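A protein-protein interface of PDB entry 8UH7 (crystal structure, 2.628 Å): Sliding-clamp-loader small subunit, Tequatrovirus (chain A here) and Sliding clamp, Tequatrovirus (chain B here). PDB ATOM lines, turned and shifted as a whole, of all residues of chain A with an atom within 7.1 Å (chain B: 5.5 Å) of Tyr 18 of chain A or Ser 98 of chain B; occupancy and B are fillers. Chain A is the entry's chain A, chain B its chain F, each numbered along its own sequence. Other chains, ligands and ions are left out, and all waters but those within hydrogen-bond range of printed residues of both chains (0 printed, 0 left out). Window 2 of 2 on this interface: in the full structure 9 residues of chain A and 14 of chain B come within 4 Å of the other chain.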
ATOM      1  N   LEU A  10     -14.462  23.325  20.118  1.00  0.00           N
ATOM      2  CA  LEU A  10     -15.481  23.895  20.981  1.00  0.00           C
ATOM      3  C   LEU A  10     -15.841  22.924  22.099  1.00  0.00           C
ATOM      4  O   LEU A  10     -15.576  21.722  22.023  1.00  0.00           O
ATOM      5  CB  LEU A  10     -16.729  24.234  20.165  1.00  0.00           C
ATOM      6  CG  LEU A  10     -16.490  24.872  18.796  1.00  0.00           C
ATOM      7  CD1 LEU A  10     -17.797  25.026  18.036  1.00  0.00           C
ATOM      8  CD2 LEU A  10     -15.794  26.213  18.948  1.00  0.00           C
ATOM      9  N   ASN A  11     -16.455  23.463  23.151  1.00  0.00           N
ATOM     10  CA  ASN A  11     -16.988  22.614  24.204  1.00  0.00           C
ATOM     11  C   ASN A  11     -18.261  21.918  23.720  1.00  0.00           C
ATOM     12  O   ASN A  11     -18.765  22.175  22.622  1.00  0.00           O
ATOM     13  CB  ASN A  11     -17.253  23.427  25.474  1.00  0.00           C
ATOM     14  CG  ASN A  11     -18.067  24.684  25.215  1.00  0.00           C
ATOM     15  OD1 ASN A  11     -18.988  24.690  24.400  1.00  0.00           O
ATOM     16  ND2 ASN A  11     -17.726  25.761  25.915  1.00  0.00           N
ATOM     17  N   GLU A  12     -18.782  21.020  24.557  1.00  0.00           N
ATOM     18  CA  GLU A  12     -19.948  20.237  24.155  1.00  0.00           C
ATOM     19  C   GLU A  12     -21.179  21.114  23.965  1.00  0.00           C
ATOM     20  O   GLU A  12     -22.014  20.825  23.099  1.00  0.00           O
ATOM     21  CB  GLU A  12     -20.224  19.140  25.183  1.00  0.00           C
ATOM     22  CG  GLU A  12     -19.143  18.069  25.241  1.00  0.00           C
ATOM     23  CD  GLU A  12     -19.447  16.984  26.253  1.00  0.00           C
ATOM     24  OE1 GLU A  12     -20.398  17.159  27.045  1.00  0.00           O
ATOM     25  OE2 GLU A  12     -18.737  15.956  26.256  1.00  0.00           O
ATOM     26  N   HIS A  13     -21.300  22.190  24.746  1.00  0.00           N
ATOM     27  CA  HIS A  13     -22.454  23.073  24.614  1.00  0.00           C
ATOM     28  C   HIS A  13     -22.458  23.785  23.266  1.00  0.00           C
ATOM     29  O   HIS A  13     -23.506  23.890  22.617  1.00  0.00           O
ATOM     30  CB  HIS A  13     -22.469  24.086  25.757  1.00  0.00           C
ATOM     31  CG  HIS A  13     -22.531  23.462  27.116  1.00  0.00           C
ATOM     32  ND1 HIS A  13     -23.678  22.880  27.615  1.00  0.00           N
ATOM     33  CD2 HIS A  13     -21.591  23.329  28.082  1.00  0.00           C
ATOM     34  CE1 HIS A  13     -23.439  22.415  28.828  1.00  0.00           C
ATOM     35  NE2 HIS A  13     -22.181  22.674  29.136  1.00  0.00           N
ATOM     36  N   GLN A  14     -21.299  24.290  22.833  1.00  0.00           N
ATOM     37  CA  GLN A  14     -21.220  24.944  21.531  1.00  0.00           C
ATOM     38  C   GLN A  14     -21.534  23.969  20.404  1.00  0.00           C
ATOM     39  O   GLN A  14     -22.250  24.313  19.457  1.00  0.00           O
ATOM     40  CB  GLN A  14     -19.836  25.557  21.331  1.00  0.00           C
ATOM     41  CG  GLN A  14     -19.581  26.809  22.140  1.00  0.00           C
ATOM     42  CD  GLN A  14     -18.168  27.328  21.964  1.00  0.00           C
ATOM     43  OE1 GLN A  14     -17.218  26.780  22.525  1.00  0.00           O
ATOM     44  NE2 GLN A  14     -18.022  28.386  21.175  1.00  0.00           N
ATOM     45  N   VAL A  15     -21.001  22.748  20.485  1.00  0.00           N
ATOM     46  CA  VAL A  15     -21.274  21.755  19.451  1.00  0.00           C
ATOM     47  C   VAL A  15     -22.757  21.416  19.421  1.00  0.00           C
ATOM     48  O   VAL A  15     -23.344  21.226  18.349  1.00  0.00           O
ATOM     49  CB  VAL A  15     -20.407  20.500  19.670  1.00  0.00           C
ATOM     50  CG1 VAL A  15     -20.703  19.451  18.607  1.00  0.00           C
ATOM     51  CG2 VAL A  15     -18.934  20.869  19.663  1.00  0.00           C
ATOM     52  N   ALA A  16     -23.391  21.351  20.594  1.00  0.00           N
ATOM     53  CA  ALA A  16     -24.811  21.018  20.648  1.00  0.00           C
ATOM     54  C   ALA A  16     -25.669  22.143  20.081  1.00  0.00           C
ATOM     55  O   ALA A  16     -26.627  21.888  19.341  1.00  0.00           O
ATOM     56  CB  ALA A  16     -25.223  20.703  22.084  1.00  0.00           C
ATOM     57  N   TRP A  17     -25.340  23.393  20.412  1.00  0.00           N
ATOM     58  CA  TRP A  17     -26.184  24.513  20.009  1.00  0.00           C
ATOM     59  C   TRP A  17     -25.966  24.892  18.547  1.00  0.00           C
ATOM     60  O   TRP A  17     -26.931  25.047  17.792  1.00  0.00           O
ATOM     61  CB  TRP A  17     -25.934  25.714  20.924  1.00  0.00           C
ATOM     62  CG  TRP A  17     -26.678  25.634  22.227  1.00  0.00           C
ATOM     63  CD1 TRP A  17     -26.204  25.167  23.419  1.00  0.00           C
ATOM     64  CD2 TRP A  17     -28.034  26.028  22.464  1.00  0.00           C
ATOM     65  NE1 TRP A  17     -27.179  25.249  24.384  1.00  0.00           N
ATOM     66  CE2 TRP A  17     -28.312  25.775  23.823  1.00  0.00           C
ATOM     67  CE3 TRP A  17     -29.040  26.573  21.660  1.00  0.00           C
ATOM     68  CZ2 TRP A  17     -29.555  26.048  24.394  1.00  0.00           C
ATOM     69  CZ3 TRP A  17     -30.273  26.841  22.228  1.00  0.00           C
ATOM     70  CH2 TRP A  17     -30.519  26.579  23.582  1.00  0.00           C
ATOM     71  N   TYR A  18     -24.707  25.046  18.129  1.00  0.00           N
ATOM     72  CA  TYR A  18     -24.429  25.459  16.757  1.00  0.00           C
ATOM     73  C   TYR A  18     -24.946  24.434  15.754  1.00  0.00           C
ATOM     74  O   TYR A  18     -25.410  24.798  14.667  1.00  0.00           O
ATOM     75  CB  TYR A  18     -22.929  25.682  16.568  1.00  0.00           C
ATOM     76  CG  TYR A  18     -22.341  26.745  17.468  1.00  0.00           C
ATOM     77  CD1 TYR A  18     -23.128  27.773  17.971  1.00  0.00           C
ATOM     78  CD2 TYR A  18     -20.998  26.719  17.813  1.00  0.00           C
ATOM     79  CE1 TYR A  18     -22.588  28.747  18.795  1.00  0.00           C
ATOM     80  CE2 TYR A  18     -20.451  27.686  18.634  1.00  0.00           C
ATOM     81  CZ  TYR A  18     -21.250  28.695  19.123  1.00  0.00           C
ATOM     82  OH  TYR A  18     -20.703  29.655  19.940  1.00  0.00           O
ATOM     83  N   SER A  19     -24.870  23.147  16.099  1.00  0.00           N
ATOM     84  CA  SER A  19     -25.431  22.106  15.246  1.00  0.00           C
ATOM     85  C   SER A  19     -26.948  22.053  15.315  1.00  0.00           C
ATOM     86  O   SER A  19     -27.573  21.459  14.429  1.00  0.00           O
ATOM     87  CB  SER A  19     -24.859  20.739  15.626  1.00  0.00           C
ATOM     88  OG  SER A  19     -25.116  20.434  16.986  1.00  0.00           O
ATOM     89  N   LYS A  20     -27.544  22.658  16.343  1.00  0.00           N
ATOM     90  CA  LYS A  20     -28.992  22.650  16.546  1.00  0.00           C
ATOM     91  C   LYS A  20     -29.540  21.230  16.651  1.00  0.00           C
ATOM     92  O   LYS A  20     -30.684  20.963  16.272  1.00  0.00           O
ATOM     93  CB  LYS A  20     -29.712  23.431  15.445  1.00  0.00           C
ATOM     94  CG  LYS A  20     -29.245  24.869  15.321  1.00  0.00           C
ATOM     95  CD  LYS A  20     -29.928  25.569  14.164  1.00  0.00           C
ATOM     96  CE  LYS A  20     -29.281  26.910  13.874  1.00  0.00           C
ATOM     97  NZ  LYS A  20     -27.823  26.792  13.577  1.00  0.00           N
ATOM     98  N   ASP A  21     -28.727  20.308  17.160  1.00  0.00           N
ATOM     99  CA  ASP A  21     -29.186  18.963  17.499  1.00  0.00           C
ATOM    100  C   ASP A  21     -29.754  19.031  18.909  1.00  0.00           C
ATOM    101  O   ASP A  21     -29.011  19.020  19.893  1.00  0.00           O
ATOM    102  CB  ASP A  21     -28.054  17.951  17.395  1.00  0.00           C
ATOM    103  CG  ASP A  21     -28.495  16.553  17.768  1.00  0.00           C
ATOM    104  OD1 ASP A  21     -29.250  15.938  16.986  1.00  0.00           O
ATOM    105  OD2 ASP A  21     -28.095  16.073  18.848  1.00  0.00           O
ATOM    106  N   VAL A  25     -28.530  19.134  22.994  1.00  0.00           N
ATOM    107  CA  VAL A  25     -28.833  20.284  23.841  1.00  0.00           C
ATOM    108  C   VAL A  25     -29.549  19.837  25.109  1.00  0.00           C
ATOM    109  O   VAL A  25     -29.267  20.331  26.208  1.00  0.00           O
ATOM    110  CB  VAL A  25     -29.659  21.319  23.055  1.00  0.00           C
ATOM    111  CG1 VAL A  25     -29.941  22.538  23.913  1.00  0.00           C
ATOM    112  CG2 VAL A  25     -28.930  21.716  21.782  1.00  0.00           C
ATOM    113  N   ASN B  18     -25.098  20.904   7.868  1.00  0.00           N
ATOM    114  CA  ASN B  18     -24.989  22.012   8.805  1.00  0.00           C
ATOM    115  C   ASN B  18     -26.205  22.908   8.625  1.00  0.00           C
ATOM    116  O   ASN B  18     -26.613  23.190   7.496  1.00  0.00           O
ATOM    117  CB  ASN B  18     -23.695  22.806   8.581  1.00  0.00           C
ATOM    118  CG  ASN B  18     -23.401  23.782   9.708  1.00  0.00           C
ATOM    119  OD1 ASN B  18     -24.292  24.178  10.460  1.00  0.00           O
ATOM    120  ND2 ASN B  18     -22.139  24.182   9.825  1.00  0.00           N
ATOM    121  N   SER B  19     -26.785  23.346   9.746  1.00  0.00           N
ATOM    122  CA  SER B  19     -27.944  24.228   9.678  1.00  0.00           C
ATOM    123  C   SER B  19     -27.574  25.598   9.122  1.00  0.00           C
ATOM    124  O   SER B  19     -28.419  26.271   8.519  1.00  0.00           O
ATOM    125  CB  SER B  19     -28.579  24.366  11.060  1.00  0.00           C
ATOM    126  OG  SER B  19     -27.620  24.776  12.020  1.00  0.00           O
ATOM    127  N   VAL B  34     -20.443  20.411  12.386  1.00  0.00           N
ATOM    128  CA  VAL B  34     -19.899  21.064  13.570  1.00  0.00           C
ATOM    129  C   VAL B  34     -18.844  20.186  14.226  1.00  0.00           C
ATOM    130  O   VAL B  34     -17.849  20.693  14.761  1.00  0.00           O
ATOM    131  CB  VAL B  34     -21.034  21.429  14.542  1.00  0.00           C
ATOM    132  CG1 VAL B  34     -20.528  22.370  15.623  1.00  0.00           C
ATOM    133  CG2 VAL B  34     -22.184  22.056  13.778  1.00  0.00           C
ATOM    134  N   ASP B  96     -23.870  36.243  12.716  1.00  0.00           N
ATOM    135  CA  ASP B  96     -22.519  36.515  13.180  1.00  0.00           C
ATOM    136  C   ASP B  96     -21.624  35.311  12.889  1.00  0.00           C
ATOM    137  O   ASP B  96     -22.039  34.166  13.093  1.00  0.00           O
ATOM    138  CB  ASP B  96     -22.521  36.819  14.677  1.00  0.00           C
ATOM    139  CG  ASP B  96     -21.175  37.298  15.178  1.00  0.00           C
ATOM    140  OD1 ASP B  96     -20.824  38.470  14.919  1.00  0.00           O
ATOM    141  OD2 ASP B  96     -20.468  36.503  15.830  1.00  0.00           O
ATOM    142  N   PRO B  97     -20.402  35.537  12.399  1.00  0.00           N
ATOM    143  CA  PRO B  97     -19.546  34.399  12.022  1.00  0.00           C
ATOM    144  C   PRO B  97     -19.173  33.493  13.184  1.00  0.00           C
ATOM    145  O   PRO B  97     -18.900  32.305  12.967  1.00  0.00           O
ATOM    146  CB  PRO B  97     -18.308  35.081  11.421  1.00  0.00           C
ATOM    147  CG  PRO B  97     -18.783  36.436  11.001  1.00  0.00           C
ATOM    148  CD  PRO B  97     -19.809  36.829  12.018  1.00  0.00           C
ATOM    149  N   SER B  98     -19.153  34.009  14.415  1.00  0.00           N
ATOM    150  CA  SER B  98     -18.755  33.193  15.555  1.00  0.00           C
ATOM    151  C   SER B  98     -19.825  32.193  15.975  1.00  0.00           C
ATOM    152  O   SER B  98     -19.543  31.328  16.812  1.00  0.00           O
ATOM    153  CB  SER B  98     -18.391  34.088  16.743  1.00  0.00           C
ATOM    154  OG  SER B  98     -19.499  34.872  17.150  1.00  0.00           O
ATOM    155  N   THR B  99     -21.036  32.284  15.423  1.00  0.00           N
ATOM    156  CA  THR B  99     -22.119  31.378  15.778  1.00  0.00           C
ATOM    157  C   THR B  99     -22.388  30.315  14.720  1.00  0.00           C
ATOM    158  O   THR B  99     -23.182  29.402  14.970  1.00  0.00           O
ATOM    159  CB  THR B  99     -23.405  32.169  16.043  1.00  0.00           C
ATOM    160  OG1 THR B  99     -23.803  32.854  14.850  1.00  0.00           O
ATOM    161  CG2 THR B  99     -23.180  33.181  17.153  1.00  0.00           C
ATOM    162  N   VAL B 100     -21.757  30.412  13.552  1.00  0.00           N
ATOM    163  CA  VAL B 100     -21.823  29.380  12.526  1.00  0.00           C
ATOM    164  C   VAL B 100     -20.421  28.828  12.314  1.00  0.00           C
ATOM    165  O   VAL B 100     -19.440  29.580  12.313  1.00  0.00           O
ATOM    166  CB  VAL B 100     -22.409  29.914  11.202  1.00  0.00           C
ATOM    167  CG1 VAL B 100     -23.888  30.223  11.365  1.00  0.00           C
ATOM    168  CG2 VAL B 100     -21.655  31.150  10.741  1.00  0.00           C
ATOM    169  N   VAL B 101     -20.330  27.511  12.158  1.00  0.00           N
ATOM    170  CA  VAL B 101     -19.061  26.832  11.927  1.00  0.00           C
ATOM    171  C   VAL B 101     -18.897  26.611  10.432  1.00  0.00           C
ATOM    172  O   VAL B 101     -19.787  26.060   9.772  1.00  0.00           O
ATOM    173  CB  VAL B 101     -18.985  25.503  12.698  1.00  0.00           C
ATOM    174  CG1 VAL B 101     -18.652  25.759  14.160  1.00  0.00           C
ATOM    175  CG2 VAL B 101     -20.295  24.752  12.579  1.00  0.00           C
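The backbone carbonyl oxygen (O) of Tyr 18 of chain A sits at hydrogen-bond distance from the side-chain hydroxyl (OG) of Ser 19 of chain B. NZ of Lys 20 of chain A sits at hydrogen-bond distance from OG of Ser 19 of chain B, 2.6 Å away.
The side-chain hydroxyl (OH) of Tyr 18 of chain A is in hydrogen-bond range of the side-chain amide nitrogen (NE2) of Gln 14 of chain A. OG of Ser 19 of chain A lies within hydrogen-bond range of O of Ala 16 of chain A. NZ of Lys 20 of chain A sits at hydrogen-bond distance from O of Tyr 18 of chain A, at 3.3 Å. OD2 of Asp 96 of chain B sits at hydrogen-bond distance from N of Ser 98 of chain B, 3.2 Å away. The backbone carbonyl oxygen of Asp 96 of chain B is in hydrogen-bond range of the side-chain hydroxyl of Thr 99 of chain B, at 2.8 Å.
Among the printed residues, pairs that only touch across the chains: Tyr 18 of chain A with Thr 99 of chain B, Ser 19 of chain A with Val 34 of chain B, Tyr 18 of chain A with Ser 98 of chain B and Val 15 of chain A with Val 34 of chain B.
Tyr 18 of chain A touches three residues of chain B. Of the printed residues of chain A, Ser 98 of chain B touches Tyr 18. Of the printed residues of chain B, Lys 20 of chain A touches Ser 19 (2.6 Å). Printed residues of chain B within 4 Å of Ser 19 of chain A: Val 34 (3.5 Å). Of the printed residues of chain A, Ser 19 of chain B touches Tyr 18 (3.4 Å) and Lys 20 (2.6 Å). Of the printed residues of chain A, Val 34 of chain B touches Val 15 (3.9 Å) and Ser 19 (3.5 Å). Of the printed residues of chain A, Thr 99 of chain B touches Tyr 18 (3.4 Å). Trp 17 of chain A touches none of the printed residues of chain B. Ala 16 of chain A touches none of the printed residues of chain B. The nearest residue of chain A that does not touch Ser 98 of chain B is Gln 14 of chain A (5.5 Å).
Hydrophobic or aromatic side chains of chain A within 4 Å of the printed part of chain B: Tyr 18. Among the printed residues, 6 pairs touch across the chains.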
